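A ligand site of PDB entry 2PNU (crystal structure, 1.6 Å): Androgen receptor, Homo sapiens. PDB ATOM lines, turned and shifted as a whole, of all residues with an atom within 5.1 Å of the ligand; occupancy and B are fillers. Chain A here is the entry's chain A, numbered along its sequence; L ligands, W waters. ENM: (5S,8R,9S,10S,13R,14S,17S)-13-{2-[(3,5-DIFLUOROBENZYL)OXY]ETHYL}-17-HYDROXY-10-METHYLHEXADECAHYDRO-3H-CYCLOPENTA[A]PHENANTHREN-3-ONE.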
ATOM      1  N   LEU A  48      13.775  -6.538  21.302  1.00  0.00           N
ATOM      2  CA  LEU A  48      12.377  -6.296  21.628  1.00  0.00           C
ATOM      3  C   LEU A  48      11.994  -4.817  21.528  1.00  0.00           C
ATOM      4  O   LEU A  48      10.860  -4.485  21.215  1.00  0.00           O
ATOM      5  CB  LEU A  48      12.036  -6.853  23.021  1.00  0.00           C
ATOM      6  CG  LEU A  48      11.596  -8.322  23.026  1.00  0.00           C
ATOM      7  CD1 LEU A  48      10.258  -8.461  22.290  1.00  0.00           C
ATOM      8  CD2 LEU A  48      12.644  -9.202  22.351  1.00  0.00           C
ATOM      9  N   LEU A  51      11.328  -4.333  18.000  1.00  0.00           N
ATOM     10  CA  LEU A  51      10.075  -4.971  17.615  1.00  0.00           C
ATOM     11  C   LEU A  51       8.918  -4.086  18.072  1.00  0.00           C
ATOM     12  O   LEU A  51       7.921  -3.939  17.375  1.00  0.00           O
ATOM     13  CB  LEU A  51       9.942  -6.375  18.229  1.00  0.00           C
ATOM     14  CG  LEU A  51      10.749  -7.494  17.564  1.00  0.00           C
ATOM     15  CD1 LEU A  51      10.649  -8.754  18.427  1.00  0.00           C
ATOM     16  CD2 LEU A  51      10.225  -7.765  16.166  1.00  0.00           C
ATOM     17  N   ASN A  52       9.051  -3.486  19.263  1.00  0.00           N
ATOM     18  CA  ASN A  52       7.994  -2.617  19.752  1.00  0.00           C
ATOM     19  C   ASN A  52       7.869  -1.366  18.892  1.00  0.00           C
ATOM     20  O   ASN A  52       6.769  -0.898  18.621  1.00  0.00           O
ATOM     21  CB  ASN A  52       8.226  -2.222  21.210  1.00  0.00           C
ATOM     22  CG  ASN A  52       7.776  -3.289  22.174  1.00  0.00           C
ATOM     23  OD1 ASN A  52       6.860  -4.053  21.885  1.00  0.00           O
ATOM     24  ND2 ASN A  52       8.409  -3.349  23.343  1.00  0.00           N
ATOM     25  N   LEU A  54       8.662  -1.172  15.760  1.00  0.00           N
ATOM     26  CA  LEU A  54       8.082  -1.636  14.508  1.00  0.00           C
ATOM     27  C   LEU A  54       6.575  -1.794  14.737  1.00  0.00           C
ATOM     28  O   LEU A  54       5.768  -1.441  13.875  1.00  0.00           O
ATOM     29  CB  LEU A  54       8.689  -2.988  14.109  1.00  0.00           C
ATOM     30  CG  LEU A  54       8.045  -3.668  12.893  1.00  0.00           C
ATOM     31  CD1 LEU A  54       8.176  -2.763  11.674  1.00  0.00           C
ATOM     32  CD2 LEU A  54       8.708  -5.027  12.635  1.00  0.00           C
ATOM     33  N   GLY A  55       6.221  -2.318  15.900  1.00  0.00           N
ATOM     34  CA  GLY A  55       4.823  -2.515  16.231  1.00  0.00           C
ATOM     35  C   GLY A  55       4.047  -1.221  16.177  1.00  0.00           C
ATOM     36  O   GLY A  55       2.973  -1.142  15.586  1.00  0.00           O
ATOM     37  N   GLN A  58       3.662  -0.174  12.576  1.00  0.00           N
ATOM     38  CA  GLN A  58       2.731  -1.063  11.873  1.00  0.00           C
ATOM     39  C   GLN A  58       1.277  -0.806  12.264  1.00  0.00           C
ATOM     40  O   GLN A  58       0.388  -0.903  11.430  1.00  0.00           O
ATOM     41  CB  GLN A  58       3.072  -2.527  12.146  1.00  0.00           C
ATOM     42  CG  GLN A  58       4.229  -3.070  11.314  1.00  0.00           C
ATOM     43  CD  GLN A  58       3.839  -3.321   9.866  1.00  0.00           C
ATOM     44  OE1 GLN A  58       2.669  -3.194   9.490  1.00  0.00           O
ATOM     45  NE2 GLN A  58       4.811  -3.694   9.048  1.00  0.00           N
ATOM     46  N   LEU A  59       1.045  -0.477  13.531  1.00  0.00           N
ATOM     47  CA  LEU A  59      -0.324  -0.207  13.972  1.00  0.00           C
ATOM     48  C   LEU A  59      -0.874   1.013  13.243  1.00  0.00           C
ATOM     49  O   LEU A  59      -2.041   1.040  12.851  1.00  0.00           O
ATOM     50  CB  LEU A  59      -0.384   0.002  15.482  1.00  0.00           C
ATOM     51  CG  LEU A  59      -1.796   0.230  16.036  1.00  0.00           C
ATOM     52  CD1 LEU A  59      -2.736  -0.903  15.616  1.00  0.00           C
ATOM     53  CD2 LEU A  59      -1.722   0.325  17.554  1.00  0.00           C
ATOM     54  N   GLN A  85      -7.750  -3.674  16.831  1.00  0.00           N
ATOM     55  CA  GLN A  85      -6.871  -4.076  17.916  1.00  0.00           C
ATOM     56  C   GLN A  85      -6.898  -5.572  18.251  1.00  0.00           C
ATOM     57  O   GLN A  85      -5.872  -6.145  18.593  1.00  0.00           O
ATOM     58  CB  GLN A  85      -7.151  -3.215  19.140  1.00  0.00           C
ATOM     59  CG  GLN A  85      -6.884  -1.749  18.837  1.00  0.00           C
ATOM     60  CD  GLN A  85      -7.196  -0.820  19.984  1.00  0.00           C
ATOM     61  OE1 GLN A  85      -8.042  -1.108  20.815  1.00  0.00           O
ATOM     62  NE2 GLN A  85      -6.522   0.334  20.006  1.00  0.00           N
ATOM     63  N   TRP A  88      -5.147  -7.348  15.120  1.00  0.00           N
ATOM     64  CA  TRP A  88      -3.797  -6.888  14.789  1.00  0.00           C
ATOM     65  C   TRP A  88      -2.675  -7.919  14.843  1.00  0.00           C
ATOM     66  O   TRP A  88      -1.912  -8.050  13.881  1.00  0.00           O
ATOM     67  CB  TRP A  88      -3.419  -5.698  15.673  1.00  0.00           C
ATOM     68  CG  TRP A  88      -2.167  -5.000  15.227  1.00  0.00           C
ATOM     69  CD1 TRP A  88      -2.045  -4.126  14.189  1.00  0.00           C
ATOM     70  CD2 TRP A  88      -0.880  -5.085  15.839  1.00  0.00           C
ATOM     71  NE1 TRP A  88      -0.755  -3.653  14.113  1.00  0.00           N
ATOM     72  CE2 TRP A  88      -0.019  -4.227  15.113  1.00  0.00           C
ATOM     73  CE3 TRP A  88      -0.357  -5.806  16.922  1.00  0.00           C
ATOM     74  CZ2 TRP A  88       1.337  -4.070  15.446  1.00  0.00           C
ATOM     75  CZ3 TRP A  88       0.990  -5.647  17.255  1.00  0.00           C
ATOM     76  CH2 TRP A  88       1.822  -4.779  16.521  1.00  0.00           C
ATOM     77  N   MET A  89      -2.558  -8.648  15.942  1.00  0.00           N
ATOM     78  CA  MET A  89      -1.476  -9.630  16.062  1.00  0.00           C
ATOM     79  C   MET A  89      -1.541 -10.638  14.922  1.00  0.00           C
ATOM     80  O   MET A  89      -0.519 -10.935  14.287  1.00  0.00           O
ATOM     81  CB  MET A  89      -1.531 -10.352  17.403  1.00  0.00           C
ATOM     82  CG  MET A  89      -0.229 -11.093  17.739  1.00  0.00           C
ATOM     83  SD  MET A  89       1.195 -10.006  18.018  1.00  0.00           S
ATOM     84  CE  MET A  89       0.841  -9.468  19.720  1.00  0.00           C
ATOM     85  N   MET A  92      -0.507  -9.103  11.631  1.00  0.00           N
ATOM     86  CA  MET A  92       0.931  -8.907  11.566  1.00  0.00           C
ATOM     87  C   MET A  92       1.720 -10.202  11.417  1.00  0.00           C
ATOM     88  O   MET A  92       2.755 -10.223  10.745  1.00  0.00           O
ATOM     89  CB  MET A  92       1.398  -8.135  12.805  1.00  0.00           C
ATOM     90  CG  MET A  92       0.818  -6.729  12.873  1.00  0.00           C
ATOM     91  SD  MET A  92       1.337  -5.695  11.476  1.00  0.00           S
ATOM     92  CE  MET A  92       0.029  -5.975  10.282  1.00  0.00           C
ATOM     93  N   VAL A  93       1.246 -11.273  12.043  1.00  0.00           N
ATOM     94  CA  VAL A  93       1.914 -12.566  11.924  1.00  0.00           C
ATOM     95  C   VAL A  93       1.787 -13.067  10.488  1.00  0.00           C
ATOM     96  O   VAL A  93       2.763 -13.537   9.893  1.00  0.00           O
ATOM     97  CB  VAL A  93       1.284 -13.615  12.876  1.00  0.00           C
ATOM     98  CG1 VAL A  93       1.711 -15.013  12.470  1.00  0.00           C
ATOM     99  CG2 VAL A  93       1.710 -13.328  14.313  1.00  0.00           C
ATOM    100  N   MET A  96       3.874 -10.765   8.127  1.00  0.00           N
ATOM    101  CA  MET A  96       5.300 -11.017   8.308  1.00  0.00           C
ATOM    102  C   MET A  96       5.668 -12.351   7.690  1.00  0.00           C
ATOM    103  O   MET A  96       6.727 -12.487   7.077  1.00  0.00           O
ATOM    104  CB  MET A  96       5.657 -10.985   9.803  1.00  0.00           C
ATOM    105  CG  MET A  96       7.155 -11.000  10.082  1.00  0.00           C
ATOM    106  SD  MET A  96       7.870 -12.661  10.087  1.00  0.00           S
ATOM    107  CE  MET A  96       7.234 -13.271  11.665  1.00  0.00           C
ATOM    108  N   ARG A  99       5.982 -11.788   4.002  1.00  0.00           N
ATOM    109  CA  ARG A  99       7.213 -11.062   3.704  1.00  0.00           C
ATOM    110  C   ARG A  99       8.411 -12.004   3.749  1.00  0.00           C
ATOM    111  O   ARG A  99       9.327 -11.907   2.931  1.00  0.00           O
ATOM    112  CB  ARG A  99       7.446  -9.930   4.719  1.00  0.00           C
ATOM    113  CG  ARG A  99       6.528  -8.742   4.588  1.00  0.00           C
ATOM    114  CD  ARG A  99       7.127  -7.529   5.299  1.00  0.00           C
ATOM    115  NE  ARG A  99       7.209  -7.684   6.752  1.00  0.00           N
ATOM    116  CZ  ARG A  99       6.167  -7.555   7.575  1.00  0.00           C
ATOM    117  NH1 ARG A  99       4.956  -7.278   7.091  1.00  0.00           N
ATOM    118  NH2 ARG A  99       6.329  -7.681   8.885  1.00  0.00           N
ATOM    119  N   PHE A 111      10.874  -9.415   9.700  1.00  0.00           N
ATOM    120  CA  PHE A 111       9.998  -8.478  10.386  1.00  0.00           C
ATOM    121  C   PHE A 111       9.993  -7.147   9.646  1.00  0.00           C
ATOM    122  O   PHE A 111       8.955  -6.507   9.501  1.00  0.00           O
ATOM    123  CB  PHE A 111      10.444  -8.265  11.838  1.00  0.00           C
ATOM    124  CG  PHE A 111      10.271  -9.476  12.703  1.00  0.00           C
ATOM    125  CD1 PHE A 111      11.336 -10.340  12.944  1.00  0.00           C
ATOM    126  CD2 PHE A 111       9.016  -9.779  13.248  1.00  0.00           C
ATOM    127  CE1 PHE A 111      11.158 -11.499  13.712  1.00  0.00           C
ATOM    128  CE2 PHE A 111       8.828 -10.935  14.017  1.00  0.00           C
ATOM    129  CZ  PHE A 111       9.904 -11.796  14.249  1.00  0.00           C
ATOM    130  N   MET A 127      12.106 -15.526  22.078  1.00  0.00           N
ATOM    131  CA  MET A 127      10.866 -15.753  21.376  1.00  0.00           C
ATOM    132  C   MET A 127      11.050 -16.876  20.358  1.00  0.00           C
ATOM    133  O   MET A 127      10.354 -16.932  19.348  1.00  0.00           O
ATOM    134  CB  MET A 127      10.474 -14.440  20.681  1.00  0.00           C
ATOM    135  CG  MET A 127       9.014 -14.294  20.322  1.00  0.00           C
ATOM    136  SD  MET A 127       8.630 -12.564  19.932  1.00  0.00           S
ATOM    137  CE  MET A 127       9.266 -12.439  18.281  1.00  0.00           C
ATOM    138  N   MET A 134       5.889 -19.083  13.559  1.00  0.00           N
ATOM    139  CA  MET A 134       5.751 -18.064  12.539  1.00  0.00           C
ATOM    140  C   MET A 134       6.500 -18.458  11.263  1.00  0.00           C
ATOM    141  O   MET A 134       6.020 -18.211  10.153  1.00  0.00           O
ATOM    142  CB  MET A 134       6.234 -16.706  13.061  1.00  0.00           C
ATOM    143  CG  MET A 134       5.326 -16.125  14.135  1.00  0.00           C
ATOM    144  SD  MET A 134       5.679 -14.414  14.542  1.00  0.00           S
ATOM    145  CE  MET A 134       7.059 -14.618  15.680  1.00  0.00           C
ATOM    146  N   LEU A 220       1.665 -15.127  20.962  1.00  0.00           N
ATOM    147  CA  LEU A 220       2.285 -13.808  20.968  1.00  0.00           C
ATOM    148  C   LEU A 220       1.540 -12.877  21.922  1.00  0.00           C
ATOM    149  O   LEU A 220       2.139 -12.014  22.538  1.00  0.00           O
ATOM    150  CB  LEU A 220       2.323 -13.233  19.543  1.00  0.00           C
ATOM    151  CG  LEU A 220       3.401 -13.877  18.665  1.00  0.00           C
ATOM    152  CD1 LEU A 220       3.294 -13.327  17.261  1.00  0.00           C
ATOM    153  CD2 LEU A 220       4.784 -13.616  19.256  1.00  0.00           C
ATOM    154  N   HIS A 221       0.226 -13.067  22.035  1.00  0.00           N
ATOM    155  CA  HIS A 221      -0.571 -12.261  22.952  1.00  0.00           C
ATOM    156  C   HIS A 221      -0.087 -12.551  24.368  1.00  0.00           C
ATOM    157  O   HIS A 221       0.111 -11.643  25.178  1.00  0.00           O
ATOM    158  CB  HIS A 221      -2.051 -12.608  22.835  1.00  0.00           C
ATOM    159  CG  HIS A 221      -2.733 -11.970  21.665  1.00  0.00           C
ATOM    160  ND1 HIS A 221      -3.661 -12.628  20.885  1.00  0.00           N
ATOM    161  CD2 HIS A 221      -2.640 -10.712  21.157  1.00  0.00           C
ATOM    162  CE1 HIS A 221      -4.110 -11.804  19.956  1.00  0.00           C
ATOM    163  NE2 HIS A 221      -3.511 -10.642  20.098  1.00  0.00           N
ATOM    164  N   PHE A 223       2.847 -13.802  25.257  1.00  0.00           N
ATOM    165  CA  PHE A 223       4.216 -13.322  25.369  1.00  0.00           C
ATOM    166  C   PHE A 223       4.285 -11.820  25.587  1.00  0.00           C
ATOM    167  O   PHE A 223       4.994 -11.347  26.472  1.00  0.00           O
ATOM    168  CB  PHE A 223       5.007 -13.712  24.111  1.00  0.00           C
ATOM    169  CG  PHE A 223       6.460 -13.330  24.166  1.00  0.00           C
ATOM    170  CD1 PHE A 223       6.883 -12.062  23.769  1.00  0.00           C
ATOM    171  CD2 PHE A 223       7.413 -14.243  24.605  1.00  0.00           C
ATOM    172  CE1 PHE A 223       8.221 -11.698  23.828  1.00  0.00           C
ATOM    173  CE2 PHE A 223       8.760 -13.895  24.667  1.00  0.00           C
ATOM    174  CZ  PHE A 223       9.172 -12.630  24.280  1.00  0.00           C
ATOM    175  N   THR A 224       3.547 -11.054  24.793  1.00  0.00           N
ATOM    176  CA  THR A 224       3.575  -9.606  24.938  1.00  0.00           C
ATOM    177  C   THR A 224       2.966  -9.177  26.268  1.00  0.00           C
ATOM    178  O   THR A 224       3.456  -8.237  26.892  1.00  0.00           O
ATOM    179  CB  THR A 224       2.863  -8.899  23.763  1.00  0.00           C
ATOM    180  OG1 THR A 224       3.162  -7.497  23.790  1.00  0.00           O
ATOM    181  CG2 THR A 224       1.365  -9.091  23.839  1.00  0.00           C
ATOM    182  N   LEU A 227       5.478  -9.881  28.920  1.00  0.00           N
ATOM    183  CA  LEU A 227       6.594  -8.965  28.771  1.00  0.00           C
ATOM    184  C   LEU A 227       6.261  -7.584  29.326  1.00  0.00           C
ATOM    185  O   LEU A 227       7.108  -6.949  29.943  1.00  0.00           O
ATOM    186  CB  LEU A 227       7.000  -8.861  27.294  1.00  0.00           C
ATOM    187  CG  LEU A 227       8.281  -8.081  27.010  1.00  0.00           C
ATOM    188  CD1 LEU A 227       9.417  -8.598  27.882  1.00  0.00           C
ATOM    189  CD2 LEU A 227       8.628  -8.217  25.529  1.00  0.00           C
ATOM    190  N   PHE A 238       8.279  -0.187  26.386  1.00  0.00           N
ATOM    191  CA  PHE A 238       6.995  -0.183  25.674  1.00  0.00           C
ATOM    192  C   PHE A 238       6.447   1.232  25.499  1.00  0.00           C
ATOM    193  O   PHE A 238       6.278   1.961  26.467  1.00  0.00           O
ATOM    194  CB  PHE A 238       5.920  -0.989  26.420  1.00  0.00           C
ATOM    195  CG  PHE A 238       6.019  -2.463  26.242  1.00  0.00           C
ATOM    196  CD1 PHE A 238       6.870  -3.217  27.040  1.00  0.00           C
ATOM    197  CD2 PHE A 238       5.249  -3.110  25.288  1.00  0.00           C
ATOM    198  CE1 PHE A 238       6.945  -4.599  26.895  1.00  0.00           C
ATOM    199  CE2 PHE A 238       5.312  -4.494  25.130  1.00  0.00           C
ATOM    200  CZ  PHE A 238       6.165  -5.245  25.942  1.00  0.00           C
ATOM    201  N   MET A 242       1.139   1.448  23.137  1.00  0.00           N
ATOM    202  CA  MET A 242       1.165  -0.010  23.084  1.00  0.00           C
ATOM    203  C   MET A 242       0.827  -0.604  24.442  1.00  0.00           C
ATOM    204  O   MET A 242       0.076  -1.572  24.545  1.00  0.00           O
ATOM    205  CB  MET A 242       2.557  -0.514  22.661  1.00  0.00           C
ATOM    206  CG  MET A 242       2.969  -0.135  21.242  1.00  0.00           C
ATOM    207  SD  MET A 242       1.972  -0.914  19.963  1.00  0.00           S
ATOM    208  CE  MET A 242       0.864   0.413  19.564  1.00  0.00           C
ATOM    209  N   ILE A 245      -2.961  -0.467  25.020  1.00  0.00           N
ATOM    210  CA  ILE A 245      -3.681  -1.476  24.254  1.00  0.00           C
ATOM    211  C   ILE A 245      -3.440  -2.877  24.811  1.00  0.00           C
ATOM    212  O   ILE A 245      -4.359  -3.688  24.909  1.00  0.00           O
ATOM    213  CB  ILE A 245      -3.258  -1.451  22.763  1.00  0.00           C
ATOM    214  CG1 ILE A 245      -3.642  -0.107  22.149  1.00  0.00           C
ATOM    215  CG2 ILE A 245      -3.917  -2.588  22.026  1.00  0.00           C
ATOM    216  CD1 ILE A 245      -3.141   0.072  20.714  1.00  0.00           C
ATOM    217  N   ILE A 246      -2.195  -3.162  25.186  1.00  0.00           N
ATOM    218  CA  ILE A 246      -1.859  -4.477  25.732  1.00  0.00           C
ATOM    219  C   ILE A 246      -2.535  -4.713  27.083  1.00  0.00           C
ATOM    220  O   ILE A 246      -2.987  -5.819  27.368  1.00  0.00           O
ATOM    221  CB  ILE A 246      -0.328  -4.639  25.894  1.00  0.00           C
ATOM    222  CG1 ILE A 246       0.346  -4.591  24.518  1.00  0.00           C
ATOM    223  CG2 ILE A 246      -0.009  -5.964  26.589  1.00  0.00           C
ATOM    224  CD1 ILE A 246       1.850  -4.459  24.570  1.00  0.00           C
ATOM    225  N   VAL A 250      -5.569  -6.975  25.196  1.00  0.00           N
ATOM    226  CA  VAL A 250      -4.995  -8.318  25.217  1.00  0.00           C
ATOM    227  C   VAL A 250      -5.568  -9.235  26.304  1.00  0.00           C
ATOM    228  O   VAL A 250      -5.810 -10.417  26.054  1.00  0.00           O
ATOM    229  CB  VAL A 250      -3.453  -8.270  25.313  1.00  0.00           C
ATOM    230  CG1 VAL A 250      -2.888  -9.680  25.385  1.00  0.00           C
ATOM    231  CG2 VAL A 250      -2.897  -7.548  24.087  1.00  0.00           C
ATOM    232  N   ILE A 253      -8.679 -11.078  25.407  1.00  0.00           N
ATOM    233  CA  ILE A 253      -8.424 -12.245  24.567  1.00  0.00           C
ATOM    234  C   ILE A 253      -7.931 -13.410  25.411  1.00  0.00           C
ATOM    235  O   ILE A 253      -8.459 -14.520  25.319  1.00  0.00           O
ATOM    236  CB  ILE A 253      -7.356 -11.904  23.499  1.00  0.00           C
ATOM    237  CG1 ILE A 253      -7.878 -10.784  22.601  1.00  0.00           C
ATOM    238  CG2 ILE A 253      -7.011 -13.156  22.707  1.00  0.00           C
ATOM    239  CD1 ILE A 253      -6.859 -10.260  21.600  1.00  0.00           C
HETATM  240  C23 ENM L   1      -0.866  -3.978  19.691  1.00  0.00           C
HETATM  241  C24 ENM L   1      -2.235  -4.156  19.393  1.00  0.00           C
HETATM  242  F2  ENM L   1      -2.926  -3.196  18.714  1.00  0.00           F
HETATM  243  C25 ENM L   1      -2.887  -5.334  19.773  1.00  0.00           C
HETATM  244  C26 ENM L   1      -2.185  -6.352  20.426  1.00  0.00           C
HETATM  245  F1  ENM L   1      -2.805  -7.503  20.754  1.00  0.00           F
HETATM  246  C27 ENM L   1      -0.819  -6.183  20.719  1.00  0.00           C
HETATM  247  C22 ENM L   1      -0.155  -4.998  20.345  1.00  0.00           C
HETATM  248  C21 ENM L   1       1.218  -4.899  20.558  1.00  0.00           C
HETATM  249  O03 ENM L   1       1.986  -6.112  20.603  1.00  0.00           O
HETATM  250  C20 ENM L   1       3.391  -5.879  20.547  1.00  0.00           C
HETATM  251  C19 ENM L   1       4.052  -7.258  20.359  1.00  0.00           C
HETATM  252  C12 ENM L   1       5.609  -7.168  20.127  1.00  0.00           C
HETATM  253  C13 ENM L   1       6.013  -5.961  19.238  1.00  0.00           C
HETATM  254  C14 ENM L   1       5.375  -6.123  17.819  1.00  0.00           C
HETATM  255  C10 ENM L   1       5.800  -7.470  17.149  1.00  0.00           C
HETATM  256  C05 ENM L   1       5.228  -7.654  15.708  1.00  0.00           C
HETATM  257  C18 ENM L   1       3.674  -7.678  15.746  1.00  0.00           C
HETATM  258  C06 ENM L   1       5.719  -6.470  14.810  1.00  0.00           C
HETATM  259  C01 ENM L   1       5.301  -6.635  13.333  1.00  0.00           C
HETATM  260  C02 ENM L   1       5.695  -8.019  12.803  1.00  0.00           C
HETATM  261  O02 ENM L   1       6.281  -8.149  11.723  1.00  0.00           O
HETATM  262  C03 ENM L   1       5.375  -9.260  13.664  1.00  0.00           C
HETATM  263  C04 ENM L   1       5.788  -9.002  15.130  1.00  0.00           C
HETATM  264  C07 ENM L   1       5.415 -10.205  16.023  1.00  0.00           C
HETATM  265  C08 ENM L   1       5.976 -10.017  17.442  1.00  0.00           C
HETATM  266  C09 ENM L   1       5.454  -8.700  18.075  1.00  0.00           C
HETATM  267  C11 ENM L   1       6.105  -8.448  19.445  1.00  0.00           C
HETATM  268  C15 ENM L   1       5.949  -9.537  20.509  1.00  0.00           C
HETATM  269  C16 ENM L   1       6.333  -8.796  21.818  1.00  0.00           C
HETATM  270  C17 ENM L   1       6.351  -7.282  21.458  1.00  0.00           C
HETATM  271  O01 ENM L   1       5.770  -6.483  22.492  1.00  0.00           O
HETATM  272  O   HOH W   1       3.679  -7.654   9.991  1.00  0.00           O
HETATM  273  O   HOH W   2      -4.317  -8.491  18.296  1.00  0.00           O
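Water W2 lies within hydrogen-bond range of the backbone carbonyl oxygen (O) of Gln 85 (2.8 Å), a ring nitrogen (NE2) of His 221 (2.9 Å), the backbone NH (N) of Met 89 (2.9 Å) and the backbone NH (N) of Trp 88 (3.5 Å).
Water W1 lies within hydrogen-bond range of the backbone carbonyl oxygen (O) of Met 92 (2.8 Å), the guanidinium group (NH2) of Arg 99 (2.9 Å) and an oxygen (O02) of the ligand (3.2 Å).
F1 of the ligand lies close to NE2 of His 221 (3.3 Å).
Residues that only touch the ligand: Gln 85 (3.3 Å), Val 250 (3.3 Å), Phe 238 (3.3 Å), Leu 51 (3.3 Å), Trp 88 (3.4 Å), Met 96 (3.4 Å), Ile 245 (3.5 Å), Phe 111 (3.5 Å), Met 89 (3.7 Å), Met 92 (3.7 Å), Leu 54 (3.8 Å), Phe 223 (3.8 Å), Leu 59 (3.9 Å), Leu 48 (3.97 Å), Leu 220 (3.97 Å) and Gly 55 (3.98 Å).
Hydrophobic or aromatic side chains within 4 Å of the ligand: Leu 48, Leu 54, Leu 59, Trp 88, Met 89, Met 92, Met 96, Phe 111, Leu 220, His 221, Phe 223, Phe 238, Ile 245 and Val 250.
The nearest printed residue that does not touch the ligand is Ile 246 (4.1 Å).
O01 of the ligand is in hydrogen-bond range of OD1 of Asn 52, at 2.7 Å.
NH2 of Arg 99 lies within hydrogen-bond range of O02 of the ligand (2.9 Å).
The side-chain hydroxyl of Thr 224 lies within hydrogen-bond range of an oxygen (O01) of the ligand (3.1 Å).
ND2 of Asn 52 lies within hydrogen-bond range of O of Leu 48 (3.4 Å).
The guanidinium group (NH2) of Arg 99 lies within hydrogen-bond range of the backbone carbonyl oxygen (O) of Phe 111.
The side-chain amide oxygen (OE1) of Gln 58 lies close to the side-chain sulfur (SD) of Met 92 (3.5 Å).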
